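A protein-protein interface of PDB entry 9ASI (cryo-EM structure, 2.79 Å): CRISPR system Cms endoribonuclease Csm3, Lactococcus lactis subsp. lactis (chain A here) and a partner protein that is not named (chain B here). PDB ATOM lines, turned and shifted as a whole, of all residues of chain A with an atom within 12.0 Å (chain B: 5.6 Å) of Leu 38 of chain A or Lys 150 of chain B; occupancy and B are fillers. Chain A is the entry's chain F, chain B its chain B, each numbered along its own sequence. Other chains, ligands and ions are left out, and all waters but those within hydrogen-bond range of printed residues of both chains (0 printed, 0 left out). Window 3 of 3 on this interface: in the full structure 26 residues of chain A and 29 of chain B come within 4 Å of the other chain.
Among the printed residues, merely in contact across the chains: Leu 38 of chain A with Phe 149 of chain B (3.2 Å), Thr 37 of chain A with Lys 124 of chain B (3.3 Å), Leu 38 of chain A with Lys 150 of chain B (3.6 Å), Leu 38 of chain A with Lys 124 of chain B (3.7 Å) and Leu 38 of chain A with Gly 123 of chain B (3.7 Å).
Of chain A, only Leu 38 comes within 4 Å of Lys 150 of chain B.
No residue of chain A comes within 4 Å of Asn 121 of chain B.
Printed residues of chain A within 4 Å of Lys 124 of chain B: Thr 37 (3.3 Å) and Leu 38 (3.7 Å).
Of the printed residues of chain A, Thr 148 of chain B touches Thr 37 (3.4 Å).
Printed residues of chain A within 4 Å of Phe 149 of chain B: Leu 38.
No residue of chain A comes within 4 Å of Glu 151 of chain B.
No residue of chain A comes within 4 Å of Asn 152 of chain B.
Thr 153 of chain B touches none of the printed residues of chain A.
Gly 154 of chain B touches none of the printed residues of chain A.
Printed residues of chain B within 4 Å of Thr 37 of chain A: Lys 124 (3.3 Å) and Thr 148 (3.4 Å).
The nearest residue of chain B that does not touch Leu 38 of chain A is Thr 148 of chain B (4.1 Å).
The nearest printed residue of chain A that does not touch Lys 150 of chain B is Thr 39 of chain A (7.8 Å).
The side-chain hydroxyl of Thr 148 of chain B is in hydrogen-bond range of the side-chain hydroxyl of Thr 37 of chain A (3.4 Å).
OD1 of Asn 121 of chain B lies within hydrogen-bond range of NZ of Lys 150 of chain B, 2.4 Å away.
The backbone NH (N) of Lys 124 of chain B sits at hydrogen-bond distance from the backbone carbonyl oxygen (O) of Thr 148 of chain B, at 3.3 Å.
Along chain A the printed residues that touch a printed residue of chain B span positions 37 to 38.
Of the 11 printed residues of chain B, 5 touch a printed residue of chain A.
Printed residues of chain B that touch a printed residue of chain A: Gly 123, Lys 124, Thr 148, Phe 149 and Lys 150.
Among the printed residues, 6 pairs touch across the chains.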
ATOM      1  N   SER A  20     -22.232  11.126  35.761  1.00  0.00           N
ATOM      2  CA  SER A  20     -22.879  12.221  36.476  1.00  0.00           C
ATOM      3  C   SER A  20     -24.006  11.610  37.301  1.00  0.00           C
ATOM      4  O   SER A  20     -25.065  11.271  36.766  1.00  0.00           O
ATOM      5  CB  SER A  20     -23.392  13.281  35.505  1.00  0.00           C
ATOM      6  OG  SER A  20     -24.309  12.724  34.580  1.00  0.00           O
ATOM      7  N   ASP A  22     -27.006  11.412  39.223  1.00  0.00           N
ATOM      8  CA  ASP A  22     -28.244  12.116  39.536  1.00  0.00           C
ATOM      9  C   ASP A  22     -29.390  11.465  38.774  1.00  0.00           C
ATOM     10  O   ASP A  22     -29.185  10.873  37.710  1.00  0.00           O
ATOM     11  CB  ASP A  22     -28.161  13.609  39.182  1.00  0.00           C
ATOM     12  CG  ASP A  22     -27.772  13.848  37.736  1.00  0.00           C
ATOM     13  OD1 ASP A  22     -27.285  12.903  37.081  1.00  0.00           O
ATOM     14  OD2 ASP A  22     -27.957  14.984  37.253  1.00  0.00           O
ATOM     15  N   VAL A  33     -24.003   9.462  30.732  1.00  0.00           N
ATOM     16  CA  VAL A  33     -22.823  10.003  30.079  1.00  0.00           C
ATOM     17  C   VAL A  33     -22.680  11.473  30.452  1.00  0.00           C
ATOM     18  O   VAL A  33     -23.603  12.104  30.973  1.00  0.00           O
ATOM     19  CB  VAL A  33     -22.880   9.824  28.548  1.00  0.00           C
ATOM     20  CG1 VAL A  33     -23.012   8.360  28.198  1.00  0.00           C
ATOM     21  CG2 VAL A  33     -24.032  10.615  27.964  1.00  0.00           C
ATOM     22  N   VAL A  34     -21.492  12.019  30.190  1.00  0.00           N
ATOM     23  CA  VAL A  34     -21.250  13.429  30.459  1.00  0.00           C
ATOM     24  C   VAL A  34     -21.955  14.276  29.410  1.00  0.00           C
ATOM     25  O   VAL A  34     -21.968  13.945  28.217  1.00  0.00           O
ATOM     26  CB  VAL A  34     -19.744  13.738  30.496  1.00  0.00           C
ATOM     27  CG1 VAL A  34     -19.135  13.230  31.778  1.00  0.00           C
ATOM     28  CG2 VAL A  34     -19.051  13.137  29.296  1.00  0.00           C
ATOM     29  N   ARG A  35     -22.545  15.377  29.855  1.00  0.00           N
ATOM     30  CA  ARG A  35     -23.294  16.271  28.993  1.00  0.00           C
ATOM     31  C   ARG A  35     -22.889  17.705  29.295  1.00  0.00           C
ATOM     32  O   ARG A  35     -22.209  17.987  30.284  1.00  0.00           O
ATOM     33  CB  ARG A  35     -24.801  16.094  29.188  1.00  0.00           C
ATOM     34  CG  ARG A  35     -25.300  14.713  28.836  1.00  0.00           C
ATOM     35  CD  ARG A  35     -26.756  14.556  29.190  1.00  0.00           C
ATOM     36  NE  ARG A  35     -27.301  13.318  28.654  1.00  0.00           N
ATOM     37  CZ  ARG A  35     -27.704  13.162  27.401  1.00  0.00           C
ATOM     38  NH1 ARG A  35     -27.615  14.144  26.521  1.00  0.00           N
ATOM     39  NH2 ARG A  35     -28.208  11.993  27.023  1.00  0.00           N
ATOM     40  N   ASP A  36     -23.299  18.614  28.419  1.00  0.00           N
ATOM     41  CA  ASP A  36     -23.129  20.028  28.699  1.00  0.00           C
ATOM     42  C   ASP A  36     -23.984  20.420  29.894  1.00  0.00           C
ATOM     43  O   ASP A  36     -25.067  19.875  30.116  1.00  0.00           O
ATOM     44  CB  ASP A  36     -23.505  20.872  27.487  1.00  0.00           C
ATOM     45  CG  ASP A  36     -22.511  20.740  26.359  1.00  0.00           C
ATOM     46  OD1 ASP A  36     -21.808  19.711  26.305  1.00  0.00           O
ATOM     47  OD2 ASP A  36     -22.430  21.666  25.525  1.00  0.00           O
ATOM     48  N   THR A  37     -23.472  21.356  30.688  1.00  0.00           N
ATOM     49  CA  THR A  37     -24.207  21.774  31.873  1.00  0.00           C
ATOM     50  C   THR A  37     -25.493  22.499  31.510  1.00  0.00           C
ATOM     51  O   THR A  37     -26.497  22.372  32.220  1.00  0.00           O
ATOM     52  CB  THR A  37     -23.330  22.660  32.750  1.00  0.00           C
ATOM     53  OG1 THR A  37     -22.017  22.093  32.831  1.00  0.00           O
ATOM     54  CG2 THR A  37     -23.913  22.750  34.140  1.00  0.00           C
ATOM     55  N   LEU A  38     -25.490  23.255  30.412  1.00  0.00           N
ATOM     56  CA  LEU A  38     -26.656  24.031  30.011  1.00  0.00           C
ATOM     57  C   LEU A  38     -27.453  23.347  28.905  1.00  0.00           C
ATOM     58  O   LEU A  38     -28.638  23.052  29.083  1.00  0.00           O
ATOM     59  CB  LEU A  38     -26.215  25.435  29.577  1.00  0.00           C
ATOM     60  CG  LEU A  38     -25.659  26.317  30.697  1.00  0.00           C
ATOM     61  CD1 LEU A  38     -25.582  27.753  30.244  1.00  0.00           C
ATOM     62  CD2 LEU A  38     -26.505  26.199  31.952  1.00  0.00           C
ATOM     63  N   THR A  39     -26.819  23.072  27.766  1.00  0.00           N
ATOM     64  CA  THR A  39     -27.528  22.503  26.627  1.00  0.00           C
ATOM     65  C   THR A  39     -27.805  21.015  26.776  1.00  0.00           C
ATOM     66  O   THR A  39     -28.604  20.474  26.003  1.00  0.00           O
ATOM     67  CB  THR A  39     -26.741  22.742  25.336  1.00  0.00           C
ATOM     68  OG1 THR A  39     -25.587  21.897  25.315  1.00  0.00           O
ATOM     69  CG2 THR A  39     -26.301  24.193  25.241  1.00  0.00           C
ATOM     70  N   ARG A  40     -27.163  20.345  27.731  1.00  0.00           N
ATOM     71  CA  ARG A  40     -27.316  18.920  28.012  1.00  0.00           C
ATOM     72  C   ARG A  40     -26.864  18.034  26.857  1.00  0.00           C
ATOM     73  O   ARG A  40     -27.060  16.815  26.908  1.00  0.00           O
ATOM     74  CB  ARG A  40     -28.758  18.572  28.400  1.00  0.00           C
ATOM     75  CG  ARG A  40     -29.131  18.984  29.810  1.00  0.00           C
ATOM     76  CD  ARG A  40     -28.501  18.062  30.836  1.00  0.00           C
ATOM     77  NE  ARG A  40     -27.323  18.663  31.450  1.00  0.00           N
ATOM     78  CZ  ARG A  40     -26.473  18.015  32.236  1.00  0.00           C
ATOM     79  NH1 ARG A  40     -26.646  16.738  32.536  1.00  0.00           N
ATOM     80  NH2 ARG A  40     -25.425  18.665  32.732  1.00  0.00           N
ATOM     81  N   LEU A  41     -26.270  18.607  25.819  1.00  0.00           N
ATOM     82  CA  LEU A  41     -25.712  17.801  24.745  1.00  0.00           C
ATOM     83  C   LEU A  41     -24.504  17.015  25.247  1.00  0.00           C
ATOM     84  O   LEU A  41     -23.710  17.534  26.036  1.00  0.00           O
ATOM     85  CB  LEU A  41     -25.298  18.682  23.570  1.00  0.00           C
ATOM     86  CG  LEU A  41     -26.235  18.775  22.371  1.00  0.00           C
ATOM     87  CD1 LEU A  41     -27.552  19.413  22.757  1.00  0.00           C
ATOM     88  CD2 LEU A  41     -25.550  19.582  21.289  1.00  0.00           C
ATOM     89  N   PRO A  42     -24.331  15.774  24.805  1.00  0.00           N
ATOM     90  CA  PRO A  42     -23.152  15.005  25.209  1.00  0.00           C
ATOM     91  C   PRO A  42     -21.880  15.633  24.670  1.00  0.00           C
ATOM     92  O   PRO A  42     -21.879  16.351  23.669  1.00  0.00           O
ATOM     93  CB  PRO A  42     -23.384  13.619  24.598  1.00  0.00           C
ATOM     94  CG  PRO A  42     -24.782  13.615  24.092  1.00  0.00           C
ATOM     95  CD  PRO A  42     -25.217  15.023  23.903  1.00  0.00           C
ATOM     96  N   LEU A  43     -20.781  15.366  25.368  1.00  0.00           N
ATOM     97  CA  LEU A  43     -19.497  15.898  24.947  1.00  0.00           C
ATOM     98  C   LEU A  43     -18.402  14.909  25.309  1.00  0.00           C
ATOM     99  O   LEU A  43     -18.598  14.002  26.121  1.00  0.00           O
ATOM    100  CB  LEU A  43     -19.202  17.260  25.589  1.00  0.00           C
ATOM    101  CG  LEU A  43     -18.730  17.326  27.041  1.00  0.00           C
ATOM    102  CD1 LEU A  43     -18.140  18.692  27.310  1.00  0.00           C
ATOM    103  CD2 LEU A  43     -19.833  17.026  28.021  1.00  0.00           C
ATOM    104  N   ASP A  98     -12.761  21.023  25.557  1.00  0.00           N
ATOM    105  CA  ASP A  98     -13.961  20.202  25.593  1.00  0.00           C
ATOM    106  C   ASP A  98     -14.597  20.165  24.210  1.00  0.00           C
ATOM    107  O   ASP A  98     -14.691  21.186  23.527  1.00  0.00           O
ATOM    108  CB  ASP A  98     -14.955  20.737  26.623  1.00  0.00           C
ATOM    109  CG  ASP A  98     -14.729  20.160  28.006  1.00  0.00           C
ATOM    110  OD1 ASP A  98     -13.585  19.769  28.308  1.00  0.00           O
ATOM    111  OD2 ASP A  98     -15.693  20.097  28.796  1.00  0.00           O
ATOM    112  N   LYS A 100     -17.766  19.493  21.930  1.00  0.00           N
ATOM    113  CA  LYS A 100     -19.219  19.452  21.955  1.00  0.00           C
ATOM    114  C   LYS A 100     -19.750  18.668  20.763  1.00  0.00           C
ATOM    115  O   LYS A 100     -19.123  18.611  19.702  1.00  0.00           O
ATOM    116  CB  LYS A 100     -19.806  20.866  21.947  1.00  0.00           C
ATOM    117  CG  LYS A 100     -19.760  21.575  23.289  1.00  0.00           C
ATOM    118  CD  LYS A 100     -18.399  22.201  23.534  1.00  0.00           C
ATOM    119  CE  LYS A 100     -18.259  22.701  24.959  1.00  0.00           C
ATOM    120  NZ  LYS A 100     -16.867  23.141  25.239  1.00  0.00           N
ATOM    121  N   LEU A 101     -20.923  18.065  20.948  1.00  0.00           N
ATOM    122  CA  LEU A 101     -21.533  17.252  19.904  1.00  0.00           C
ATOM    123  C   LEU A 101     -21.904  18.118  18.707  1.00  0.00           C
ATOM    124  O   LEU A 101     -22.760  19.000  18.808  1.00  0.00           O
ATOM    125  CB  LEU A 101     -22.761  16.531  20.449  1.00  0.00           C
ATOM    126  CG  LEU A 101     -23.418  15.503  19.531  1.00  0.00           C
ATOM    127  CD1 LEU A 101     -22.385  14.658  18.824  1.00  0.00           C
ATOM    128  CD2 LEU A 101     -24.349  14.628  20.338  1.00  0.00           C
ATOM    129  N   LEU A 104     -26.022  17.485  15.444  1.00  0.00           N
ATOM    130  CA  LEU A 104     -27.437  17.544  15.779  1.00  0.00           C
ATOM    131  C   LEU A 104     -28.311  17.882  14.589  1.00  0.00           C
ATOM    132  O   LEU A 104     -29.433  17.385  14.505  1.00  0.00           O
ATOM    133  CB  LEU A 104     -27.697  18.561  16.897  1.00  0.00           C
ATOM    134  CG  LEU A 104     -27.647  18.038  18.334  1.00  0.00           C
ATOM    135  CD1 LEU A 104     -28.784  17.062  18.583  1.00  0.00           C
ATOM    136  CD2 LEU A 104     -26.321  17.376  18.627  1.00  0.00           C
ATOM    137  N   ASN B 121     -29.014  35.714  35.615  1.00  0.00           N
ATOM    138  CA  ASN B 121     -28.793  34.282  35.445  1.00  0.00           C
ATOM    139  C   ASN B 121     -27.820  34.092  34.294  1.00  0.00           C
ATOM    140  O   ASN B 121     -28.190  34.258  33.128  1.00  0.00           O
ATOM    141  CB  ASN B 121     -30.099  33.536  35.182  1.00  0.00           C
ATOM    142  CG  ASN B 121     -29.976  32.048  35.439  1.00  0.00           C
ATOM    143  OD1 ASN B 121     -30.067  31.238  34.517  1.00  0.00           O
ATOM    144  ND2 ASN B 121     -29.768  31.680  36.698  1.00  0.00           N
ATOM    145  N   LEU B 122     -26.579  33.750  34.621  1.00  0.00           N
ATOM    146  CA  LEU B 122     -25.557  33.450  33.625  1.00  0.00           C
ATOM    147  C   LEU B 122     -25.028  32.052  33.931  1.00  0.00           C
ATOM    148  O   LEU B 122     -24.255  31.860  34.871  1.00  0.00           O
ATOM    149  CB  LEU B 122     -24.462  34.517  33.626  1.00  0.00           C
ATOM    150  CG  LEU B 122     -23.317  34.625  34.634  1.00  0.00           C
ATOM    151  CD1 LEU B 122     -22.296  35.635  34.159  1.00  0.00           C
ATOM    152  CD2 LEU B 122     -23.836  34.976  36.004  1.00  0.00           C
ATOM    153  N   GLY B 123     -25.491  31.068  33.172  1.00  0.00           N
ATOM    154  CA  GLY B 123     -25.056  29.699  33.353  1.00  0.00           C
ATOM    155  C   GLY B 123     -25.176  29.167  34.765  1.00  0.00           C
ATOM    156  O   GLY B 123     -25.944  29.693  35.574  1.00  0.00           O
ATOM    157  N   LYS B 124     -24.417  28.117  35.071  1.00  0.00           N
ATOM    158  CA  LYS B 124     -24.481  27.506  36.388  1.00  0.00           C
ATOM    159  C   LYS B 124     -23.194  26.740  36.655  1.00  0.00           C
ATOM    160  O   LYS B 124     -22.497  26.315  35.733  1.00  0.00           O
ATOM    161  CB  LYS B 124     -25.697  26.583  36.515  1.00  0.00           C
ATOM    162  CG  LYS B 124     -25.744  25.484  35.479  1.00  0.00           C
ATOM    163  CD  LYS B 124     -27.066  24.744  35.524  1.00  0.00           C
ATOM    164  CE  LYS B 124     -27.123  23.792  36.703  1.00  0.00           C
ATOM    165  NZ  LYS B 124     -25.892  22.964  36.806  1.00  0.00           N
ATOM    166  N   THR B 148     -20.207  27.079  33.284  1.00  0.00           N
ATOM    167  CA  THR B 148     -20.522  27.334  31.884  1.00  0.00           C
ATOM    168  C   THR B 148     -21.411  28.563  31.789  1.00  0.00           C
ATOM    169  O   THR B 148     -22.373  28.690  32.546  1.00  0.00           O
ATOM    170  CB  THR B 148     -21.223  26.132  31.248  1.00  0.00           C
ATOM    171  OG1 THR B 148     -20.552  24.925  31.624  1.00  0.00           O
ATOM    172  CG2 THR B 148     -21.217  26.252  29.735  1.00  0.00           C
ATOM    173  N   PHE B 149     -21.083  29.468  30.871  1.00  0.00           N
ATOM    174  CA  PHE B 149     -21.881  30.663  30.650  1.00  0.00           C
ATOM    175  C   PHE B 149     -23.026  30.373  29.683  1.00  0.00           C
ATOM    176  O   PHE B 149     -23.088  29.320  29.046  1.00  0.00           O
ATOM    177  CB  PHE B 149     -21.019  31.799  30.100  1.00  0.00           C
ATOM    178  CG  PHE B 149     -19.910  32.228  31.014  1.00  0.00           C
ATOM    179  CD1 PHE B 149     -18.708  31.547  31.034  1.00  0.00           C
ATOM    180  CD2 PHE B 149     -20.060  33.324  31.840  1.00  0.00           C
ATOM    181  CE1 PHE B 149     -17.686  31.946  31.867  1.00  0.00           C
ATOM    182  CE2 PHE B 149     -19.040  33.723  32.673  1.00  0.00           C
ATOM    183  CZ  PHE B 149     -17.851  33.033  32.684  1.00  0.00           C
ATOM    184  N   LYS B 150     -23.940  31.335  29.567  1.00  0.00           N
ATOM    185  CA  LYS B 150     -25.060  31.226  28.641  1.00  0.00           C
ATOM    186  C   LYS B 150     -24.588  31.561  27.229  1.00  0.00           C
ATOM    187  O   LYS B 150     -23.401  31.785  26.979  1.00  0.00           O
ATOM    188  CB  LYS B 150     -26.209  32.129  29.081  1.00  0.00           C
ATOM    189  CG  LYS B 150     -26.886  31.705  30.367  1.00  0.00           C
ATOM    190  CD  LYS B 150     -27.875  30.582  30.143  1.00  0.00           C
ATOM    191  CE  LYS B 150     -28.287  29.952  31.462  1.00  0.00           C
ATOM    192  NZ  LYS B 150     -28.987  30.908  32.356  1.00  0.00           N
ATOM    193  N   GLU B 151     -25.525  31.598  26.279  1.00  0.00           N
ATOM    194  CA  GLU B 151     -25.157  31.798  24.880  1.00  0.00           C
ATOM    195  C   GLU B 151     -24.674  33.220  24.623  1.00  0.00           C
ATOM    196  O   GLU B 151     -23.627  33.427  23.999  1.00  0.00           O
ATOM    197  CB  GLU B 151     -26.339  31.457  23.975  1.00  0.00           C
ATOM    198  CG  GLU B 151     -26.679  29.980  23.943  1.00  0.00           C
ATOM    199  CD  GLU B 151     -25.594  29.151  23.285  1.00  0.00           C
ATOM    200  OE1 GLU B 151     -24.927  29.669  22.365  1.00  0.00           O
ATOM    201  OE2 GLU B 151     -25.407  27.983  23.686  1.00  0.00           O
ATOM    202  N   ASN B 152     -25.421  34.215  25.094  1.00  0.00           N
ATOM    203  CA  ASN B 152     -25.094  35.621  24.860  1.00  0.00           C
ATOM    204  C   ASN B 152     -24.477  36.260  26.093  1.00  0.00           C
ATOM    205  O   ASN B 152     -24.701  37.439  26.379  1.00  0.00           O
ATOM    206  CB  ASN B 152     -26.339  36.388  24.426  1.00  0.00           C
ATOM    207  CG  ASN B 152     -26.855  35.944  23.075  1.00  0.00           C
ATOM    208  OD1 ASN B 152     -26.092  35.807  22.119  1.00  0.00           O
ATOM    209  ND2 ASN B 152     -28.160  35.711  22.988  1.00  0.00           N
ATOM    210  N   THR B 153     -23.684  35.493  26.833  1.00  0.00           N
ATOM    211  CA  THR B 153     -23.191  35.913  28.133  1.00  0.00           C
ATOM    212  C   THR B 153     -21.712  35.579  28.242  1.00  0.00           C
ATOM    213  O   THR B 153     -21.230  34.621  27.634  1.00  0.00           O
ATOM    214  CB  THR B 153     -23.987  35.229  29.254  1.00  0.00           C
ATOM    215  OG1 THR B 153     -25.368  35.589  29.144  1.00  0.00           O
ATOM    216  CG2 THR B 153     -23.488  35.656  30.602  1.00  0.00           C
ATOM    217  N   GLY B 154     -20.993  36.388  29.014  1.00  0.00           N
ATOM    218  CA  GLY B 154     -19.597  36.130  29.299  1.00  0.00           C
ATOM    219  C   GLY B 154     -19.062  37.049  30.375  1.00  0.00           C
ATOM    220  O   GLY B 154     -19.768  37.372  31.333  1.00  0.00           O
